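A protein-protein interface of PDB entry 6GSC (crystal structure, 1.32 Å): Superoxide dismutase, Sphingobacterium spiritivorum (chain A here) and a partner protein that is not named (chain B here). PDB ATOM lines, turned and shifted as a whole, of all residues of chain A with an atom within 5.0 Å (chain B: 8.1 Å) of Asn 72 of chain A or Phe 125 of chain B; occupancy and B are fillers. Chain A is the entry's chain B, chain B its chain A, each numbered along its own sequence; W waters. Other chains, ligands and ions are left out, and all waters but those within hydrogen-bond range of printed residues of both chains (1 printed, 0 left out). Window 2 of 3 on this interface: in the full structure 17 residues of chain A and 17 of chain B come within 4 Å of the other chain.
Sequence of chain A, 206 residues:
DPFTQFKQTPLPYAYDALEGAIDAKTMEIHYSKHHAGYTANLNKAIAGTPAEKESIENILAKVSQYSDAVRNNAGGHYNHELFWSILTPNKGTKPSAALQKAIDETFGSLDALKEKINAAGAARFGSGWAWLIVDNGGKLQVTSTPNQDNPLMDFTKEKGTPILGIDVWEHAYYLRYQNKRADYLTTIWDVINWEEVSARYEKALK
The backbone carbonyl oxygen (O) of Gly 126 of chain B lies within hydrogen-bond range of the guanidinium group (NH2) of Arg 181 of chain B, 3.1 Å away. The side-chain hydroxyl (OH) of Tyr 38 of chain A lies within hydrogen-bond range of the side-chain amide nitrogen (NE2) of Gln 148 of chain A (3.1 Å). The backbone carbonyl oxygen (O) of Asp 68 of chain A lies close to the side-chain amide nitrogen (ND2) of Asn 72 of chain A (3.4 Å). The backbone carbonyl oxygen (O) of Asn 147 of chain A is in hydrogen-bond range of the indole nitrogen (NE1) of Trp 169 of chain A (2.8 Å). NE2 of Gln 148 of chain A lies close to NE1 of Trp 169 of chain A, 3.4 Å away.
Tyr 38 of chain A touches Phe 125 of chain B. CG of Asn 72 of chain A touches CD2 of Phe 125 of chain B, 3.5 Å away. Asn 147 of chain A touches Gly 126 of chain B. Phe 125 of chain B touches Gln 148 of chain A (CZ to CG, 3.6 Å). Phe 125 of chain B touches Trp 169 of chain A (CE2 to CH2, 3.9 Å). Gly 126 of chain B touches Trp 169 of chain A.
Of chain B, only Phe 125 comes within 4 Å of Asn 72 of chain A. Phe 125 of chain B touches just these residues of chain A: Tyr 38, Asn 72, Gln 148 and Trp 169. Of the printed residues of chain B, Tyr 38 of chain A touches Phe 125. Printed residues of chain B within 4 Å of Gln 148 of chain A: Phe 125. Printed residues of chain A within 4 Å of Gly 126 of chain B: Asn 147 and Trp 169. Of the printed residues of chain B, Asn 147 of chain A touches Gly 126 (3.6 Å). Of the printed residues of chain B, Trp 169 of chain A touches Phe 125 and Gly 126. Ala 122 of chain B touches none of the printed residues of chain A. Val 168 of chain B touches none of the printed residues of chain A. The nearest residue of chain A that does not touch Phe 125 of chain B is Asn 147 of chain A (4.1 Å).
Printed residues of chain B that touch a printed residue of chain A: Phe 125 and Gly 126. Hydrophobic or aromatic side chains of chain B within 4 Å of the printed part of chain A: Phe 125. Along chain B the printed residues that touch a printed residue of chain A span positions 125 to 126. Hydrophobic or aromatic side chains of chain A within 4 Å of the printed part of chain B: Tyr 38 and Trp 169. Among the printed residues, 6 pairs touch across the chains. Among the printed residues, no Asp or Glu carboxylate lies within 4 Å of a Lys or Arg side-chain nitrogen of the other chain.
Water W1 lies within hydrogen-bond range of OD1 of Asn 147 of chain A (2.8 Å), OD1 of Asn 147 of chain B (2.8 Å) and N of Ser 127 of chain B (3.0 Å).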
ATOM      1  N   TYR A  38     -30.642  -4.266  -1.486  1.00  0.00           N
ATOM      2  CA  TYR A  38     -29.929  -5.155  -0.543  1.00  0.00           C
ATOM      3  C   TYR A  38     -30.858  -6.199   0.059  1.00  0.00           C
ATOM      4  O   TYR A  38     -30.483  -7.358   0.138  1.00  0.00           O
ATOM      5  CB  TYR A  38     -29.262  -4.383   0.583  1.00  0.00           C
ATOM      6  CG  TYR A  38     -28.183  -3.397   0.121  1.00  0.00           C
ATOM      7  CD1 TYR A  38     -27.220  -3.764  -0.781  1.00  0.00           C
ATOM      8  CD2 TYR A  38     -28.122  -2.130   0.612  1.00  0.00           C
ATOM      9  CE1 TYR A  38     -26.254  -2.852  -1.209  1.00  0.00           C
ATOM     10  CE2 TYR A  38     -27.167  -1.221   0.189  1.00  0.00           C
ATOM     11  CZ  TYR A  38     -26.246  -1.625  -0.707  1.00  0.00           C
ATOM     12  OH  TYR A  38     -25.294  -0.708  -1.130  1.00  0.00           O
ATOM     13  N   ASP A  68     -20.023 -13.812  -1.366  1.00  0.00           N
ATOM     14  CA  ASP A  68     -19.945 -12.354  -1.342  1.00  0.00           C
ATOM     15  C   ASP A  68     -21.349 -11.775  -1.412  1.00  0.00           C
ATOM     16  O   ASP A  68     -21.581 -10.734  -0.794  1.00  0.00           O
ATOM     17  CB  ASP A  68     -19.114 -11.809  -2.511  1.00  0.00           C
ATOM     18  CG  ASP A  68     -17.653 -12.180  -2.433  1.00  0.00           C
ATOM     19  OD1 ASP A  68     -17.153 -12.523  -1.348  1.00  0.00           O
ATOM     20  OD2 ASP A  68     -16.996 -12.114  -3.506  1.00  0.00           O
ATOM     21  N   ALA A  69     -22.247 -12.339  -2.207  1.00  0.00           N
ATOM     22  CA  ALA A  69     -23.613 -11.819  -2.272  1.00  0.00           C
ATOM     23  C   ALA A  69     -24.279 -11.865  -0.920  1.00  0.00           C
ATOM     24  O   ALA A  69     -24.995 -10.936  -0.576  1.00  0.00           O
ATOM     25  CB  ALA A  69     -24.452 -12.532  -3.327  1.00  0.00           C
ATOM     26  N   VAL A  70     -24.075 -12.900  -0.141  1.00  0.00           N
ATOM     27  CA  VAL A  70     -24.646 -12.928   1.210  1.00  0.00           C
ATOM     28  C   VAL A  70     -24.010 -11.842   2.057  1.00  0.00           C
ATOM     29  O   VAL A  70     -24.677 -11.023   2.671  1.00  0.00           O
ATOM     30  CB  VAL A  70     -24.515 -14.329   1.859  1.00  0.00           C
ATOM     31  CG1 VAL A  70     -24.923 -14.281   3.306  1.00  0.00           C
ATOM     32  CG2 VAL A  70     -25.343 -15.346   1.107  1.00  0.00           C
ATOM     33  N   ARG A  71     -22.691 -11.763   2.069  1.00  0.00           N
ATOM     34  CA  ARG A  71     -21.991 -10.813   2.857  1.00  0.00           C
ATOM     35  C   ARG A  71     -22.438  -9.394   2.552  1.00  0.00           C
ATOM     36  O   ARG A  71     -22.740  -8.599   3.443  1.00  0.00           O
ATOM     37  CB  ARG A  71     -20.484 -10.921   2.586  1.00  0.00           C
ATOM     38  CG  ARG A  71     -19.633  -9.828   3.205  1.00  0.00           C
ATOM     39  CD  ARG A  71     -18.327  -9.746   2.494  1.00  0.00           C
ATOM     40  NE  ARG A  71     -17.395  -8.814   3.095  1.00  0.00           N
ATOM     41  CZ  ARG A  71     -16.083  -8.962   3.026  1.00  0.00           C
ATOM     42  NH1 ARG A  71     -15.552 -10.025   2.428  1.00  0.00           N
ATOM     43  NH2 ARG A  71     -15.275  -8.059   3.519  1.00  0.00           N
ATOM     44  N   ASN A  72     -22.398  -9.004   1.283  1.00  0.00           N
ATOM     45  CA  ASN A  72     -22.659  -7.635   0.908  1.00  0.00           C
ATOM     46  C   ASN A  72     -24.101  -7.240   1.176  1.00  0.00           C
ATOM     47  O   ASN A  72     -24.370  -6.109   1.582  1.00  0.00           O
ATOM     48  CB  ASN A  72     -22.283  -7.405  -0.546  1.00  0.00           C
ATOM     49  CG  ASN A  72     -20.793  -7.469  -0.772  1.00  0.00           C
ATOM     50  OD1 ASN A  72     -20.023  -7.169   0.131  1.00  0.00           O
ATOM     51  ND2 ASN A  72     -20.392  -7.808  -1.982  1.00  0.00           N
ATOM     52  N   ASN A  73     -25.028  -8.163   0.919  1.00  0.00           N
ATOM     53  CA  ASN A  73     -26.448  -7.835   1.076  1.00  0.00           C
ATOM     54  C   ASN A  73     -26.928  -8.045   2.500  1.00  0.00           C
ATOM     55  O   ASN A  73     -27.810  -7.304   2.944  1.00  0.00           O
ATOM     56  CB  ASN A  73     -27.283  -8.598   0.052  1.00  0.00           C
ATOM     57  CG  ASN A  73     -26.972  -8.144  -1.333  1.00  0.00           C
ATOM     58  OD1 ASN A  73     -27.243  -7.011  -1.681  1.00  0.00           O
ATOM     59  ND2 ASN A  73     -26.309  -9.004  -2.103  1.00  0.00           N
ATOM     60  N   ALA A  74     -26.379  -8.984   3.242  1.00  0.00           N
ATOM     61  CA  ALA A  74     -26.662  -9.058   4.680  1.00  0.00           C
ATOM     62  C   ALA A  74     -26.176  -7.820   5.402  1.00  0.00           C
ATOM     63  O   ALA A  74     -26.907  -7.242   6.188  1.00  0.00           O
ATOM     64  CB  ALA A  74     -26.039 -10.285   5.297  1.00  0.00           C
ATOM     65  N   GLY A  75     -24.960  -7.391   5.112  1.00  0.00           N
ATOM     66  CA  GLY A  75     -24.468  -6.142   5.610  1.00  0.00           C
ATOM     67  C   GLY A  75     -25.372  -5.001   5.228  1.00  0.00           C
ATOM     68  O   GLY A  75     -25.779  -4.232   6.061  1.00  0.00           O
ATOM     69  N   GLY A  76     -25.694  -4.895   3.957  1.00  0.00           N
ATOM     70  CA  GLY A  76     -26.499  -3.810   3.496  1.00  0.00           C
ATOM     71  C   GLY A  76     -27.837  -3.732   4.170  1.00  0.00           C
ATOM     72  O   GLY A  76     -28.305  -2.656   4.532  1.00  0.00           O
ATOM     73  N   ASN A 147     -17.439  -0.682   2.693  1.00  0.00           N
ATOM     74  CA  ASN A 147     -18.553  -1.211   1.931  1.00  0.00           C
ATOM     75  C   ASN A 147     -19.780  -1.434   2.836  1.00  0.00           C
ATOM     76  O   ASN A 147     -20.156  -0.474   3.526  1.00  0.00           O
ATOM     77  CB  ASN A 147     -18.143  -2.382   1.058  1.00  0.00           C
ATOM     78  CG  ASN A 147     -16.999  -1.997   0.178  1.00  0.00           C
ATOM     79  OD1 ASN A 147     -16.924  -0.896  -0.330  1.00  0.00           O
ATOM     80  ND2 ASN A 147     -16.063  -2.916   0.031  1.00  0.00           N
ATOM     81  N   GLN A 148     -20.400  -2.624   2.824  1.00  0.00           N
ATOM     82  CA  GLN A 148     -21.503  -2.871   3.767  1.00  0.00           C
ATOM     83  C   GLN A 148     -21.049  -3.766   4.905  1.00  0.00           C
ATOM     84  O   GLN A 148     -21.908  -4.347   5.604  1.00  0.00           O
ATOM     85  CB  GLN A 148     -22.714  -3.474   3.056  1.00  0.00           C
ATOM     86  CG  GLN A 148     -23.358  -2.573   2.005  1.00  0.00           C
ATOM     87  CD  GLN A 148     -23.878  -1.277   2.556  1.00  0.00           C
ATOM     88  OE1 GLN A 148     -24.037  -1.108   3.774  1.00  0.00           O
ATOM     89  NE2 GLN A 148     -24.136  -0.342   1.668  1.00  0.00           N
ATOM     90  N   ASP A 149     -19.754  -3.886   5.153  1.00  0.00           N
ATOM     91  CA  ASP A 149     -19.327  -4.632   6.292  1.00  0.00           C
ATOM     92  C   ASP A 149     -19.724  -3.937   7.571  1.00  0.00           C
ATOM     93  O   ASP A 149     -20.008  -2.748   7.580  1.00  0.00           O
ATOM     94  CB  ASP A 149     -17.834  -4.886   6.230  1.00  0.00           C
ATOM     95  CG  ASP A 149     -17.425  -5.762   5.071  1.00  0.00           C
ATOM     96  OD1 ASP A 149     -18.244  -6.343   4.373  1.00  0.00           O
ATOM     97  OD2 ASP A 149     -16.190  -5.938   4.876  1.00  0.00           O
ATOM     98  N   TRP A 169     -21.169   5.993   2.465  1.00  0.00           N
ATOM     99  CA  TRP A 169     -21.250   5.837   1.030  1.00  0.00           C
ATOM    100  C   TRP A 169     -21.631   7.175   0.401  1.00  0.00           C
ATOM    101  O   TRP A 169     -22.472   7.894   0.942  1.00  0.00           O
ATOM    102  CB  TRP A 169     -22.303   4.815   0.620  1.00  0.00           C
ATOM    103  CG  TRP A 169     -21.885   3.397   0.855  1.00  0.00           C
ATOM    104  CD1 TRP A 169     -21.560   2.798   2.038  1.00  0.00           C
ATOM    105  CD2 TRP A 169     -21.872   2.346  -0.129  1.00  0.00           C
ATOM    106  NE1 TRP A 169     -21.316   1.489   1.846  1.00  0.00           N
ATOM    107  CE2 TRP A 169     -21.470   1.169   0.533  1.00  0.00           C
ATOM    108  CE3 TRP A 169     -22.125   2.289  -1.510  1.00  0.00           C
ATOM    109  CZ2 TRP A 169     -21.328  -0.041  -0.139  1.00  0.00           C
ATOM    110  CZ3 TRP A 169     -22.022   1.112  -2.152  1.00  0.00           C
ATOM    111  CH2 TRP A 169     -21.594  -0.057  -1.466  1.00  0.00           C
ATOM    112  N   ALA B 120     -18.545  -5.715 -15.658  1.00  0.00           N
ATOM    113  CA  ALA B 120     -17.489  -5.566 -14.661  1.00  0.00           C
ATOM    114  C   ALA B 120     -17.698  -4.345 -13.786  1.00  0.00           C
ATOM    115  O   ALA B 120     -17.550  -4.390 -12.575  1.00  0.00           O
ATOM    116  CB  ALA B 120     -16.125  -5.502 -15.329  1.00  0.00           C
ATOM    117  N   GLY B 121     -18.106  -3.246 -14.413  1.00  0.00           N
ATOM    118  CA  GLY B 121     -18.436  -2.066 -13.673  1.00  0.00           C
ATOM    119  C   GLY B 121     -19.608  -2.239 -12.732  1.00  0.00           C
ATOM    120  O   GLY B 121     -19.564  -1.815 -11.584  1.00  0.00           O
ATOM    121  N   ALA B 122     -20.632  -2.902 -13.218  1.00  0.00           N
ATOM    122  CA  ALA B 122     -21.812  -3.130 -12.372  1.00  0.00           C
ATOM    123  C   ALA B 122     -21.507  -4.024 -11.217  1.00  0.00           C
ATOM    124  O   ALA B 122     -22.083  -3.866 -10.160  1.00  0.00           O
ATOM    125  CB  ALA B 122     -22.902  -3.756 -13.198  1.00  0.00           C
ATOM    126  N   ALA B 123     -20.602  -4.974 -11.393  1.00  0.00           N
ATOM    127  CA  ALA B 123     -20.262  -5.977 -10.383  1.00  0.00           C
ATOM    128  C   ALA B 123     -19.293  -5.512  -9.317  1.00  0.00           C
ATOM    129  O   ALA B 123     -19.078  -6.202  -8.342  1.00  0.00           O
ATOM    130  CB  ALA B 123     -19.706  -7.183 -11.063  1.00  0.00           C
ATOM    131  N   ARG B 124     -18.692  -4.357  -9.506  1.00  0.00           N
ATOM    132  CA  ARG B 124     -17.772  -3.824  -8.541  1.00  0.00           C
ATOM    133  C   ARG B 124     -18.588  -3.250  -7.385  1.00  0.00           C
ATOM    134  O   ARG B 124     -19.150  -2.159  -7.492  1.00  0.00           O
ATOM    135  CB  ARG B 124     -16.874  -2.785  -9.193  1.00  0.00           C
ATOM    136  CG  ARG B 124     -15.950  -2.042  -8.221  1.00  0.00           C
ATOM    137  CD  ARG B 124     -15.254  -2.959  -7.250  1.00  0.00           C
ATOM    138  NE  ARG B 124     -14.369  -3.908  -7.861  1.00  0.00           N
ATOM    139  CZ  ARG B 124     -13.565  -4.716  -7.218  1.00  0.00           C
ATOM    140  NH1 ARG B 124     -13.573  -4.683  -5.876  1.00  0.00           N
ATOM    141  NH2 ARG B 124     -12.760  -5.513  -7.857  1.00  0.00           N
ATOM    142  N   PHE B 125     -18.629  -3.947  -6.278  1.00  0.00           N
ATOM    143  CA  PHE B 125     -19.395  -3.525  -5.112  1.00  0.00           C
ATOM    144  C   PHE B 125     -18.649  -2.451  -4.376  1.00  0.00           C
ATOM    145  O   PHE B 125     -17.447  -2.600  -4.099  1.00  0.00           O
ATOM    146  CB  PHE B 125     -19.638  -4.710  -4.169  1.00  0.00           C
ATOM    147  CG  PHE B 125     -20.691  -4.439  -3.138  1.00  0.00           C
ATOM    148  CD1 PHE B 125     -22.016  -4.402  -3.505  1.00  0.00           C
ATOM    149  CD2 PHE B 125     -20.357  -4.175  -1.834  1.00  0.00           C
ATOM    150  CE1 PHE B 125     -23.001  -4.130  -2.594  1.00  0.00           C
ATOM    151  CE2 PHE B 125     -21.344  -3.920  -0.938  1.00  0.00           C
ATOM    152  CZ  PHE B 125     -22.648  -3.878  -1.299  1.00  0.00           C
ATOM    153  N   GLY B 126     -19.327  -1.359  -4.061  1.00  0.00           N
ATOM    154  CA  GLY B 126     -18.650  -0.240  -3.433  1.00  0.00           C
ATOM    155  C   GLY B 126     -18.026   0.663  -4.478  1.00  0.00           C
ATOM    156  O   GLY B 126     -18.463   0.758  -5.606  1.00  0.00           O
ATOM    157  N   SER B 127     -16.954   1.341  -4.073  1.00  0.00           N
ATOM    158  CA  SER B 127     -16.269   2.253  -4.960  1.00  0.00           C
ATOM    159  C   SER B 127     -15.226   1.513  -5.784  1.00  0.00           C
ATOM    160  O   SER B 127     -14.565   0.579  -5.299  1.00  0.00           O
ATOM    161  CB  SER B 127     -15.536   3.291  -4.148  1.00  0.00           C
ATOM    162  OG  SER B 127     -16.418   3.973  -3.265  1.00  0.00           O
ATOM    163  N   GLY B 128     -14.983   1.990  -7.000  1.00  0.00           N
ATOM    164  CA  GLY B 128     -13.899   1.423  -7.791  1.00  0.00           C
ATOM    165  C   GLY B 128     -13.931   1.789  -9.235  1.00  0.00           C
ATOM    166  O   GLY B 128     -14.549   2.803  -9.571  1.00  0.00           O
ATOM    167  N   SER B 144     -11.922  -5.209 -12.790  1.00  0.00           N
ATOM    168  CA  SER B 144     -12.252  -4.085 -11.979  1.00  0.00           C
ATOM    169  C   SER B 144     -11.407  -4.083 -10.735  1.00  0.00           C
ATOM    170  O   SER B 144     -10.860  -5.126 -10.374  1.00  0.00           O
ATOM    171  CB  SER B 144     -13.739  -4.070 -11.598  1.00  0.00           C
ATOM    172  OG  SER B 144     -14.045  -5.007 -10.572  1.00  0.00           O
ATOM    173  N   THR B 145     -11.291  -2.931 -10.114  1.00  0.00           N
ATOM    174  CA  THR B 145     -10.555  -2.769  -8.894  1.00  0.00           C
ATOM    175  C   THR B 145     -11.353  -1.974  -7.885  1.00  0.00           C
ATOM    176  O   THR B 145     -12.245  -1.174  -8.258  1.00  0.00           O
ATOM    177  CB  THR B 145      -9.217  -2.052  -9.162  1.00  0.00           C
ATOM    178  OG1 THR B 145      -9.497  -0.785  -9.745  1.00  0.00           O
ATOM    179  CG2 THR B 145      -8.268  -2.896  -9.986  1.00  0.00           C
ATOM    180  N   PRO B 146     -11.076  -2.146  -6.597  1.00  0.00           N
ATOM    181  CA  PRO B 146     -11.703  -1.356  -5.568  1.00  0.00           C
ATOM    182  C   PRO B 146     -11.055  -0.022  -5.355  1.00  0.00           C
ATOM    183  O   PRO B 146      -9.838   0.108  -5.590  1.00  0.00           O
ATOM    184  CB  PRO B 146     -11.517  -2.197  -4.323  1.00  0.00           C
ATOM    185  CG  PRO B 146     -10.208  -2.909  -4.572  1.00  0.00           C
ATOM    186  CD  PRO B 146     -10.169  -3.185  -6.059  1.00  0.00           C
ATOM    187  N   ASN B 147     -11.822   0.960  -4.941  1.00  0.00           N
ATOM    188  CA  ASN B 147     -11.327   2.197  -4.446  1.00  0.00           C
ATOM    189  C   ASN B 147     -10.466   2.884  -5.522  1.00  0.00           C
ATOM    190  O   ASN B 147     -10.971   3.040  -6.621  1.00  0.00           O
ATOM    191  CB  ASN B 147     -10.667   2.041  -3.071  1.00  0.00           C
ATOM    192  CG  ASN B 147     -11.625   1.446  -2.092  1.00  0.00           C
ATOM    193  OD1 ASN B 147     -12.817   1.786  -2.105  1.00  0.00           O
ATOM    194  ND2 ASN B 147     -11.147   0.571  -1.245  1.00  0.00           N
ATOM    195  N   VAL B 168     -16.370   4.070 -11.336  1.00  0.00           N
ATOM    196  CA  VAL B 168     -17.700   3.737 -10.818  1.00  0.00           C
ATOM    197  C   VAL B 168     -17.808   4.071  -9.364  1.00  0.00           C
ATOM    198  O   VAL B 168     -18.734   3.593  -8.706  1.00  0.00           O
ATOM    199  CB  VAL B 168     -18.097   2.291 -11.134  1.00  0.00           C
ATOM    200  CG1 VAL B 168     -18.246   2.119 -12.630  1.00  0.00           C
ATOM    201  CG2 VAL B 168     -17.163   1.269 -10.570  1.00  0.00           C
ATOM    202  N   ARG B 181     -26.320   3.148 -11.874  1.00  0.00           N
ATOM    203  CA  ARG B 181     -24.966   2.945 -12.413  1.00  0.00           C
ATOM    204  C   ARG B 181     -24.967   2.285 -13.776  1.00  0.00           C
ATOM    205  O   ARG B 181     -24.162   2.644 -14.632  1.00  0.00           O
ATOM    206  CB  ARG B 181     -24.131   2.136 -11.437  1.00  0.00           C
ATOM    207  CG  ARG B 181     -22.672   2.005 -11.849  1.00  0.00           C
ATOM    208  CD  ARG B 181     -21.882   0.951 -11.105  1.00  0.00           C
ATOM    209  NE  ARG B 181     -21.651   1.342  -9.749  1.00  0.00           N
ATOM    210  CZ  ARG B 181     -20.932   0.622  -8.900  1.00  0.00           C
ATOM    211  NH1 ARG B 181     -20.316  -0.468  -9.308  1.00  0.00           N
ATOM    212  NH2 ARG B 181     -20.813   1.015  -7.644  1.00  0.00           N
HETATM  213  O   HOH W   1     -15.473   1.158  -1.489  1.00  0.00           O
